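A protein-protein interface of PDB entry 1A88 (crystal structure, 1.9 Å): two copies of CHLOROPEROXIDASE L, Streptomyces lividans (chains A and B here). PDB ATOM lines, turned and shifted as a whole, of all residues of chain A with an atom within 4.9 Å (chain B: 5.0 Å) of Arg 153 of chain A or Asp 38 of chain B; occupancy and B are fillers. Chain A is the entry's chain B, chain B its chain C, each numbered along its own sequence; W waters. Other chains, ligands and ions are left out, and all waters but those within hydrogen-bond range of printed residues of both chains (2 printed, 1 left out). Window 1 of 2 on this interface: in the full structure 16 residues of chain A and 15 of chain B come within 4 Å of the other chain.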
ATOM      1  N   ALA A 148      -4.235  -3.444  15.817  1.00  0.00           N
ATOM      2  CA  ALA A 148      -3.893  -3.011  14.457  1.00  0.00           C
ATOM      3  C   ALA A 148      -5.155  -2.685  13.644  1.00  0.00           C
ATOM      4  O   ALA A 148      -5.136  -1.731  12.886  1.00  0.00           O
ATOM      5  CB  ALA A 148      -3.095  -4.087  13.738  1.00  0.00           C
ATOM      6  N   LEU A 149      -6.181  -3.524  13.807  1.00  0.00           N
ATOM      7  CA  LEU A 149      -7.450  -3.293  13.096  1.00  0.00           C
ATOM      8  C   LEU A 149      -8.026  -1.945  13.489  1.00  0.00           C
ATOM      9  O   LEU A 149      -8.427  -1.125  12.645  1.00  0.00           O
ATOM     10  CB  LEU A 149      -8.373  -4.484  13.380  1.00  0.00           C
ATOM     11  CG  LEU A 149      -9.716  -4.577  12.623  1.00  0.00           C
ATOM     12  CD1 LEU A 149     -10.276  -5.988  12.839  1.00  0.00           C
ATOM     13  CD2 LEU A 149     -10.741  -3.533  12.976  1.00  0.00           C
ATOM     14  N   ALA A 151      -6.496   0.699  14.706  1.00  0.00           N
ATOM     15  CA  ALA A 151      -5.638   1.816  14.355  1.00  0.00           C
ATOM     16  C   ALA A 151      -5.619   2.110  12.833  1.00  0.00           C
ATOM     17  O   ALA A 151      -5.636   3.290  12.490  1.00  0.00           O
ATOM     18  CB  ALA A 151      -4.146   1.634  14.652  1.00  0.00           C
ATOM     19  N   ASN A 152      -5.541   1.121  11.990  1.00  0.00           N
ATOM     20  CA  ASN A 152      -5.507   1.427  10.521  1.00  0.00           C
ATOM     21  C   ASN A 152      -5.970   0.188   9.788  1.00  0.00           C
ATOM     22  O   ASN A 152      -5.212  -0.708   9.415  1.00  0.00           O
ATOM     23  CB  ASN A 152      -4.063   1.788  10.112  1.00  0.00           C
ATOM     24  CG  ASN A 152      -4.010   2.232   8.652  1.00  0.00           C
ATOM     25  OD1 ASN A 152      -4.918   1.906   7.864  1.00  0.00           O
ATOM     26  ND2 ASN A 152      -2.971   2.917   8.192  1.00  0.00           N
ATOM     27  N   ARG A 153      -7.311  -0.038   9.792  1.00  0.00           N
ATOM     28  CA  ARG A 153      -7.912  -1.230   9.261  1.00  0.00           C
ATOM     29  C   ARG A 153      -7.455  -1.437   7.812  1.00  0.00           C
ATOM     30  O   ARG A 153      -7.224  -2.574   7.431  1.00  0.00           O
ATOM     31  CB  ARG A 153      -9.465  -1.139   9.317  1.00  0.00           C
ATOM     32  CG  ARG A 153     -10.159  -2.473   9.090  1.00  0.00           C
ATOM     33  CD  ARG A 153     -11.637  -2.466   9.519  1.00  0.00           C
ATOM     34  NE  ARG A 153     -12.395  -1.488   8.700  1.00  0.00           N
ATOM     35  CZ  ARG A 153     -13.413  -1.867   7.901  1.00  0.00           C
ATOM     36  NH1 ARG A 153     -13.810  -3.112   7.736  1.00  0.00           N
ATOM     37  NH2 ARG A 153     -14.009  -0.919   7.182  1.00  0.00           N
ATOM     38  N   ALA A 154      -7.459  -0.353   7.007  1.00  0.00           N
ATOM     39  CA  ALA A 154      -7.093  -0.511   5.594  1.00  0.00           C
ATOM     40  C   ALA A 154      -5.681  -1.057   5.386  1.00  0.00           C
ATOM     41  O   ALA A 154      -5.432  -1.825   4.444  1.00  0.00           O
ATOM     42  CB  ALA A 154      -7.288   0.857   4.967  1.00  0.00           C
ATOM     43  N   GLN A 155      -4.734  -0.656   6.246  1.00  0.00           N
ATOM     44  CA  GLN A 155      -3.386  -1.257   6.074  1.00  0.00           C
ATOM     45  C   GLN A 155      -3.292  -2.659   6.596  1.00  0.00           C
ATOM     46  O   GLN A 155      -2.648  -3.578   6.065  1.00  0.00           O
ATOM     47  CB  GLN A 155      -2.387  -0.344   6.806  1.00  0.00           C
ATOM     48  CG  GLN A 155      -0.934  -0.860   6.651  1.00  0.00           C
ATOM     49  CD  GLN A 155      -0.577  -0.804   5.191  1.00  0.00           C
ATOM     50  OE1 GLN A 155      -0.830   0.198   4.521  1.00  0.00           O
ATOM     51  NE2 GLN A 155      -0.060  -1.920   4.728  1.00  0.00           N
ATOM     52  N   PHE A 156      -3.922  -2.951   7.738  1.00  0.00           N
ATOM     53  CA  PHE A 156      -3.953  -4.213   8.415  1.00  0.00           C
ATOM     54  C   PHE A 156      -4.540  -5.267   7.442  1.00  0.00           C
ATOM     55  O   PHE A 156      -4.028  -6.394   7.369  1.00  0.00           O
ATOM     56  CB  PHE A 156      -4.763  -4.237   9.701  1.00  0.00           C
ATOM     57  CG  PHE A 156      -4.920  -5.528  10.436  1.00  0.00           C
ATOM     58  CD1 PHE A 156      -3.812  -6.247  10.876  1.00  0.00           C
ATOM     59  CD2 PHE A 156      -6.194  -6.042  10.700  1.00  0.00           C
ATOM     60  CE1 PHE A 156      -3.966  -7.425  11.577  1.00  0.00           C
ATOM     61  CE2 PHE A 156      -6.326  -7.212  11.419  1.00  0.00           C
ATOM     62  CZ  PHE A 156      -5.217  -7.894  11.862  1.00  0.00           C
ATOM     63  N   TYR A 157      -5.520  -4.829   6.630  1.00  0.00           N
ATOM     64  CA  TYR A 157      -6.155  -5.768   5.676  1.00  0.00           C
ATOM     65  C   TYR A 157      -5.313  -5.956   4.419  1.00  0.00           C
ATOM     66  O   TYR A 157      -5.720  -6.763   3.590  1.00  0.00           O
ATOM     67  CB  TYR A 157      -7.586  -5.313   5.326  1.00  0.00           C
ATOM     68  CG  TYR A 157      -8.602  -5.587   6.417  1.00  0.00           C
ATOM     69  CD1 TYR A 157      -8.234  -6.132   7.664  1.00  0.00           C
ATOM     70  CD2 TYR A 157      -9.948  -5.324   6.216  1.00  0.00           C
ATOM     71  CE1 TYR A 157      -9.180  -6.363   8.633  1.00  0.00           C
ATOM     72  CE2 TYR A 157     -10.905  -5.538   7.187  1.00  0.00           C
ATOM     73  CZ  TYR A 157     -10.524  -6.061   8.383  1.00  0.00           C
ATOM     74  OH  TYR A 157     -11.469  -6.323   9.339  1.00  0.00           O
ATOM     75  N   GLY A 187     -12.917  -7.422   3.047  1.00  0.00           N
ATOM     76  CA  GLY A 187     -12.838  -6.862   4.415  1.00  0.00           C
ATOM     77  C   GLY A 187     -13.225  -5.400   4.496  1.00  0.00           C
ATOM     78  O   GLY A 187     -13.989  -5.050   5.434  1.00  0.00           O
ATOM     79  N   MET A 188     -12.853  -4.514   3.577  1.00  0.00           N
ATOM     80  CA  MET A 188     -13.171  -3.109   3.661  1.00  0.00           C
ATOM     81  C   MET A 188     -14.682  -2.847   3.469  1.00  0.00           C
ATOM     82  O   MET A 188     -15.202  -1.827   3.943  1.00  0.00           O
ATOM     83  CB  MET A 188     -12.303  -2.259   2.727  1.00  0.00           C
ATOM     84  CG  MET A 188     -10.776  -2.239   3.033  1.00  0.00           C
ATOM     85  SD  MET A 188     -10.435  -2.043   4.817  1.00  0.00           S
ATOM     86  CE  MET A 188     -10.976  -0.399   5.157  1.00  0.00           C
ATOM     87  N   GLY A 190     -17.029  -4.631   4.873  1.00  0.00           N
ATOM     88  CA  GLY A 190     -17.676  -4.944   6.137  1.00  0.00           C
ATOM     89  C   GLY A 190     -17.394  -3.882   7.189  1.00  0.00           C
ATOM     90  O   GLY A 190     -16.642  -2.912   7.032  1.00  0.00           O
ATOM     91  N   ALA A 191     -18.075  -4.090   8.325  1.00  0.00           N
ATOM     92  CA  ALA A 191     -18.051  -3.094   9.421  1.00  0.00           C
ATOM     93  C   ALA A 191     -16.839  -3.228  10.373  1.00  0.00           C
ATOM     94  O   ALA A 191     -16.631  -4.345  10.883  1.00  0.00           O
ATOM     95  CB  ALA A 191     -19.335  -3.303  10.219  1.00  0.00           C
ATOM     96  N   ALA A 192     -16.266  -2.056  10.662  1.00  0.00           N
ATOM     97  CA  ALA A 192     -15.118  -2.077  11.615  1.00  0.00           C
ATOM     98  C   ALA A 192     -15.557  -2.637  12.965  1.00  0.00           C
ATOM     99  O   ALA A 192     -14.829  -3.483  13.479  1.00  0.00           O
ATOM    100  CB  ALA A 192     -14.560  -0.651  11.757  1.00  0.00           C
ATOM    101  N   HIS A 195     -16.061  -6.559  12.680  1.00  0.00           N
ATOM    102  CA  HIS A 195     -14.756  -7.247  12.503  1.00  0.00           C
ATOM    103  C   HIS A 195     -13.946  -7.193  13.813  1.00  0.00           C
ATOM    104  O   HIS A 195     -13.275  -8.195  14.103  1.00  0.00           O
ATOM    105  CB  HIS A 195     -13.944  -6.590  11.377  1.00  0.00           C
ATOM    106  CG  HIS A 195     -14.573  -6.806  10.034  1.00  0.00           C
ATOM    107  ND1 HIS A 195     -14.126  -6.195   8.895  1.00  0.00           N
ATOM    108  CD2 HIS A 195     -15.592  -7.658   9.681  1.00  0.00           C
ATOM    109  CE1 HIS A 195     -14.862  -6.621   7.870  1.00  0.00           C
ATOM    110  NE2 HIS A 195     -15.753  -7.514   8.335  1.00  0.00           N
ATOM    111  N   LYS B  14     -24.650   4.623   9.689  1.00  0.00           N
ATOM    112  CA  LYS B  14     -24.279   3.617  10.695  1.00  0.00           C
ATOM    113  C   LYS B  14     -24.657   4.245  12.065  1.00  0.00           C
ATOM    114  O   LYS B  14     -24.471   5.472  12.196  1.00  0.00           O
ATOM    115  CB  LYS B  14     -22.740   3.578  10.722  1.00  0.00           C
ATOM    116  CG  LYS B  14     -22.085   2.672   9.716  1.00  0.00           C
ATOM    117  CD  LYS B  14     -20.604   3.029   9.683  1.00  0.00           C
ATOM    118  CE  LYS B  14     -20.074   2.814   8.278  1.00  0.00           C
ATOM    119  NZ  LYS B  14     -19.187   1.597   8.322  1.00  0.00           N
ATOM    120  N   ALA B  34     -18.855   7.389   5.014  1.00  0.00           N
ATOM    121  CA  ALA B  34     -18.878   7.153   6.445  1.00  0.00           C
ATOM    122  C   ALA B  34     -17.690   6.275   6.894  1.00  0.00           C
ATOM    123  O   ALA B  34     -17.285   6.382   8.077  1.00  0.00           O
ATOM    124  CB  ALA B  34     -20.133   6.472   6.965  1.00  0.00           C
ATOM    125  N   ASP B  35     -17.192   5.451   6.009  1.00  0.00           N
ATOM    126  CA  ASP B  35     -16.117   4.507   6.299  1.00  0.00           C
ATOM    127  C   ASP B  35     -14.795   5.233   6.507  1.00  0.00           C
ATOM    128  O   ASP B  35     -13.903   4.575   7.056  1.00  0.00           O
ATOM    129  CB  ASP B  35     -15.939   3.463   5.213  1.00  0.00           C
ATOM    130  CG  ASP B  35     -17.113   2.456   5.236  1.00  0.00           C
ATOM    131  OD1 ASP B  35     -18.061   2.661   6.012  1.00  0.00           O
ATOM    132  OD2 ASP B  35     -17.066   1.561   4.372  1.00  0.00           O
ATOM    133  N   ASP B  36     -14.668   6.492   6.177  1.00  0.00           N
ATOM    134  CA  ASP B  36     -13.447   7.238   6.464  1.00  0.00           C
ATOM    135  C   ASP B  36     -13.253   7.401   7.981  1.00  0.00           C
ATOM    136  O   ASP B  36     -12.141   7.800   8.334  1.00  0.00           O
ATOM    137  CB  ASP B  36     -13.488   8.634   5.823  1.00  0.00           C
ATOM    138  CG  ASP B  36     -12.052   9.189   5.694  1.00  0.00           C
ATOM    139  OD1 ASP B  36     -11.206   8.458   5.184  1.00  0.00           O
ATOM    140  OD2 ASP B  36     -11.773  10.337   6.056  1.00  0.00           O
ATOM    141  N   TRP B  37     -14.261   7.176   8.806  1.00  0.00           N
ATOM    142  CA  TRP B  37     -14.167   7.407  10.247  1.00  0.00           C
ATOM    143  C   TRP B  37     -13.898   6.180  11.085  1.00  0.00           C
ATOM    144  O   TRP B  37     -14.050   6.196  12.334  1.00  0.00           O
ATOM    145  CB  TRP B  37     -15.555   7.949  10.696  1.00  0.00           C
ATOM    146  CG  TRP B  37     -15.812   9.346  10.170  1.00  0.00           C
ATOM    147  CD1 TRP B  37     -16.727   9.716   9.230  1.00  0.00           C
ATOM    148  CD2 TRP B  37     -15.108  10.531  10.555  1.00  0.00           C
ATOM    149  NE1 TRP B  37     -16.637  11.087   9.041  1.00  0.00           N
ATOM    150  CE2 TRP B  37     -15.664  11.605   9.831  1.00  0.00           C
ATOM    151  CE3 TRP B  37     -14.117  10.800  11.530  1.00  0.00           C
ATOM    152  CZ2 TRP B  37     -15.268  12.932  10.047  1.00  0.00           C
ATOM    153  CZ3 TRP B  37     -13.665  12.105  11.687  1.00  0.00           C
ATOM    154  CH2 TRP B  37     -14.259  13.160  10.968  1.00  0.00           C
ATOM    155  N   ASP B  38     -13.583   5.010  10.491  1.00  0.00           N
ATOM    156  CA  ASP B  38     -13.456   3.761  11.213  1.00  0.00           C
ATOM    157  C   ASP B  38     -12.623   3.958  12.519  1.00  0.00           C
ATOM    158  O   ASP B  38     -13.021   3.421  13.539  1.00  0.00           O
ATOM    159  CB  ASP B  38     -12.715   2.699  10.359  1.00  0.00           C
ATOM    160  CG  ASP B  38     -13.634   1.998   9.336  1.00  0.00           C
ATOM    161  OD1 ASP B  38     -14.891   2.162   9.338  1.00  0.00           O
ATOM    162  OD2 ASP B  38     -13.051   1.323   8.449  1.00  0.00           O
ATOM    163  N   ASN B  39     -11.439   4.563  12.401  1.00  0.00           N
ATOM    164  CA  ASN B  39     -10.590   4.712  13.603  1.00  0.00           C
ATOM    165  C   ASN B  39     -11.345   5.458  14.723  1.00  0.00           C
ATOM    166  O   ASN B  39     -11.428   4.914  15.848  1.00  0.00           O
ATOM    167  CB  ASN B  39      -9.300   5.421  13.170  1.00  0.00           C
ATOM    168  CG  ASN B  39      -8.408   5.733  14.380  1.00  0.00           C
ATOM    169  OD1 ASN B  39      -8.826   6.468  15.270  1.00  0.00           O
ATOM    170  ND2 ASN B  39      -7.213   5.116  14.388  1.00  0.00           N
ATOM    171  N   GLN B  40     -11.804   6.656  14.423  1.00  0.00           N
ATOM    172  CA  GLN B  40     -12.518   7.496  15.402  1.00  0.00           C
ATOM    173  C   GLN B  40     -13.801   6.876  15.887  1.00  0.00           C
ATOM    174  O   GLN B  40     -14.110   6.970  17.093  1.00  0.00           O
ATOM    175  CB  GLN B  40     -12.797   8.906  14.908  1.00  0.00           C
ATOM    176  CG  GLN B  40     -11.570   9.797  14.839  1.00  0.00           C
ATOM    177  CD  GLN B  40     -10.595   9.484  13.739  1.00  0.00           C
ATOM    178  OE1 GLN B  40     -11.009   8.983  12.650  1.00  0.00           O
ATOM    179  NE2 GLN B  40      -9.300   9.732  14.012  1.00  0.00           N
ATOM    180  N   MET B  41     -14.569   6.153  15.038  1.00  0.00           N
ATOM    181  CA  MET B  41     -15.710   5.425  15.567  1.00  0.00           C
ATOM    182  C   MET B  41     -15.384   4.348  16.584  1.00  0.00           C
ATOM    183  O   MET B  41     -16.060   4.301  17.652  1.00  0.00           O
ATOM    184  CB  MET B  41     -16.520   4.765  14.389  1.00  0.00           C
ATOM    185  CG  MET B  41     -17.187   6.055  13.789  1.00  0.00           C
ATOM    186  SD  MET B  41     -18.252   5.665  12.441  1.00  0.00           S
ATOM    187  CE  MET B  41     -19.697   4.897  13.114  1.00  0.00           C
ATOM    188  N   LEU B  42     -14.360   3.520  16.305  1.00  0.00           N
ATOM    189  CA  LEU B  42     -13.984   2.489  17.304  1.00  0.00           C
ATOM    190  C   LEU B  42     -13.398   3.144  18.563  1.00  0.00           C
ATOM    191  O   LEU B  42     -13.691   2.641  19.664  1.00  0.00           O
ATOM    192  CB  LEU B  42     -12.981   1.491  16.729  1.00  0.00           C
ATOM    193  CG  LEU B  42     -13.547   0.571  15.614  1.00  0.00           C
ATOM    194  CD1 LEU B  42     -12.514  -0.481  15.215  1.00  0.00           C
ATOM    195  CD2 LEU B  42     -14.829  -0.096  16.038  1.00  0.00           C
ATOM    196  N   PHE B  43     -12.664   4.219  18.395  1.00  0.00           N
ATOM    197  CA  PHE B  43     -12.115   4.945  19.565  1.00  0.00           C
ATOM    198  C   PHE B  43     -13.214   5.459  20.473  1.00  0.00           C
ATOM    199  O   PHE B  43     -13.256   5.172  21.692  1.00  0.00           O
ATOM    200  CB  PHE B  43     -11.291   6.116  19.096  1.00  0.00           C
ATOM    201  CG  PHE B  43     -10.741   7.014  20.189  1.00  0.00           C
ATOM    202  CD1 PHE B  43      -9.649   6.588  20.928  1.00  0.00           C
ATOM    203  CD2 PHE B  43     -11.303   8.239  20.456  1.00  0.00           C
ATOM    204  CE1 PHE B  43      -9.123   7.412  21.941  1.00  0.00           C
ATOM    205  CE2 PHE B  43     -10.819   9.061  21.478  1.00  0.00           C
ATOM    206  CZ  PHE B  43      -9.709   8.629  22.198  1.00  0.00           C
ATOM    207  N   HIS B 182      -7.879   2.750   0.230  1.00  0.00           N
ATOM    208  CA  HIS B 182      -9.192   2.990   0.826  1.00  0.00           C
ATOM    209  C   HIS B 182      -9.777   4.307   0.409  1.00  0.00           C
ATOM    210  O   HIS B 182     -11.026   4.406   0.234  1.00  0.00           O
ATOM    211  CB  HIS B 182      -9.116   2.914   2.392  1.00  0.00           C
ATOM    212  CG  HIS B 182     -10.463   2.674   2.978  1.00  0.00           C
ATOM    213  ND1 HIS B 182     -10.831   3.168   4.207  1.00  0.00           N
ATOM    214  CD2 HIS B 182     -11.584   2.035   2.489  1.00  0.00           C
ATOM    215  CE1 HIS B 182     -12.062   2.808   4.489  1.00  0.00           C
ATOM    216  NE2 HIS B 182     -12.573   2.133   3.445  1.00  0.00           N
HETATM  217  O   HOH W   1     -14.858   0.769   3.263  1.00  0.00           O
HETATM  218  O   HOH W   2     -17.812  -0.581   6.233  1.00  0.00           O
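The side-chain carboxylate (OD2) of Asp 38 of chain B lies within salt-bridge range of the guanidinium group (NH2) of Arg 153 of chain A (2.7 Å).
ND2 of Asn 39 of chain B lies within hydrogen-bond range of O of Ala 151 of chain A (3.1 Å).
NZ of Lys 14 of chain B is in salt-bridge range of OD1 of Asp 35 of chain B (2.8 Å).
NH1 of Arg 153 of chain A sits at hydrogen-bond distance from O of Gly 187 of chain A, 3.0 Å away.
A ring nitrogen (ND1) of His 195 of chain A sits at hydrogen-bond distance from the guanidinium group of Arg 153 of chain A, at 3.3 Å.
O of Gly 190 of chain A sits at hydrogen-bond distance from NH1 of Arg 153 of chain A (2.9 Å).
No position is printed for both chains.
Of the 6 pairs that touch across the chains among the printed residues, none has its exchanged pair printed and touching as well.
Water W1 lies within hydrogen-bond range of the side-chain carboxylate (OD2) of Asp 35 of chain B, a ring nitrogen (NE2) of His 182 of chain B and the backbone carbonyl oxygen (O) of Met 188 of chain A.
Water W2 lies within hydrogen-bond range of O of Gly 190 of chain A (2.7 Å), OD2 of Asp 35 of chain B (2.9 Å) and NZ of Lys 14 of chain B (3.3 Å).
Asp 38 of chain B touches just these residues of chain A: Arg 153 (2.7 Å) and Ala 192 (3.7 Å).
Of the printed residues of chain B, Ala 154 of chain A touches His 182.
Of the printed residues of chain B, Ala 192 of chain A touches Asp 38 (3.7 Å).
Tyr 157 of chain A touches none of the printed residues of chain B.
Asp 36 of chain B touches none of the printed residues of chain A.
The nearest residue of chain B that does not touch Arg 153 of chain A is Asp 35 of chain B (4.8 Å).
The nearest printed residue of chain B that does not touch Ala 151 of chain A is Leu 42 of chain B (6.2 Å).
Among the printed residues, merely in contact across the chains: Ala 154 of chain A with His 182 of chain B (3.8 Å), Met 188 of chain A with Asp 35 of chain B (3.9 Å), Met 188 of chain A with His 182 of chain B (3.4 Å) and Ala 192 of chain A with Asp 38 of chain B (3.7 Å).
Printed residues of chain B that touch a printed residue of chain A: Asp 35, Asp 38, Asn 39 and His 182.
Hydrophobic or aromatic side chains of chain B within 4 Å of the printed part of chain A: His 182.
Hydrophobic or aromatic side chains of chain A within 4 Å of the printed part of chain B: Ala 154, Met 188 and Ala 192.
Among the printed residues, 6 pairs touch across the chains.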
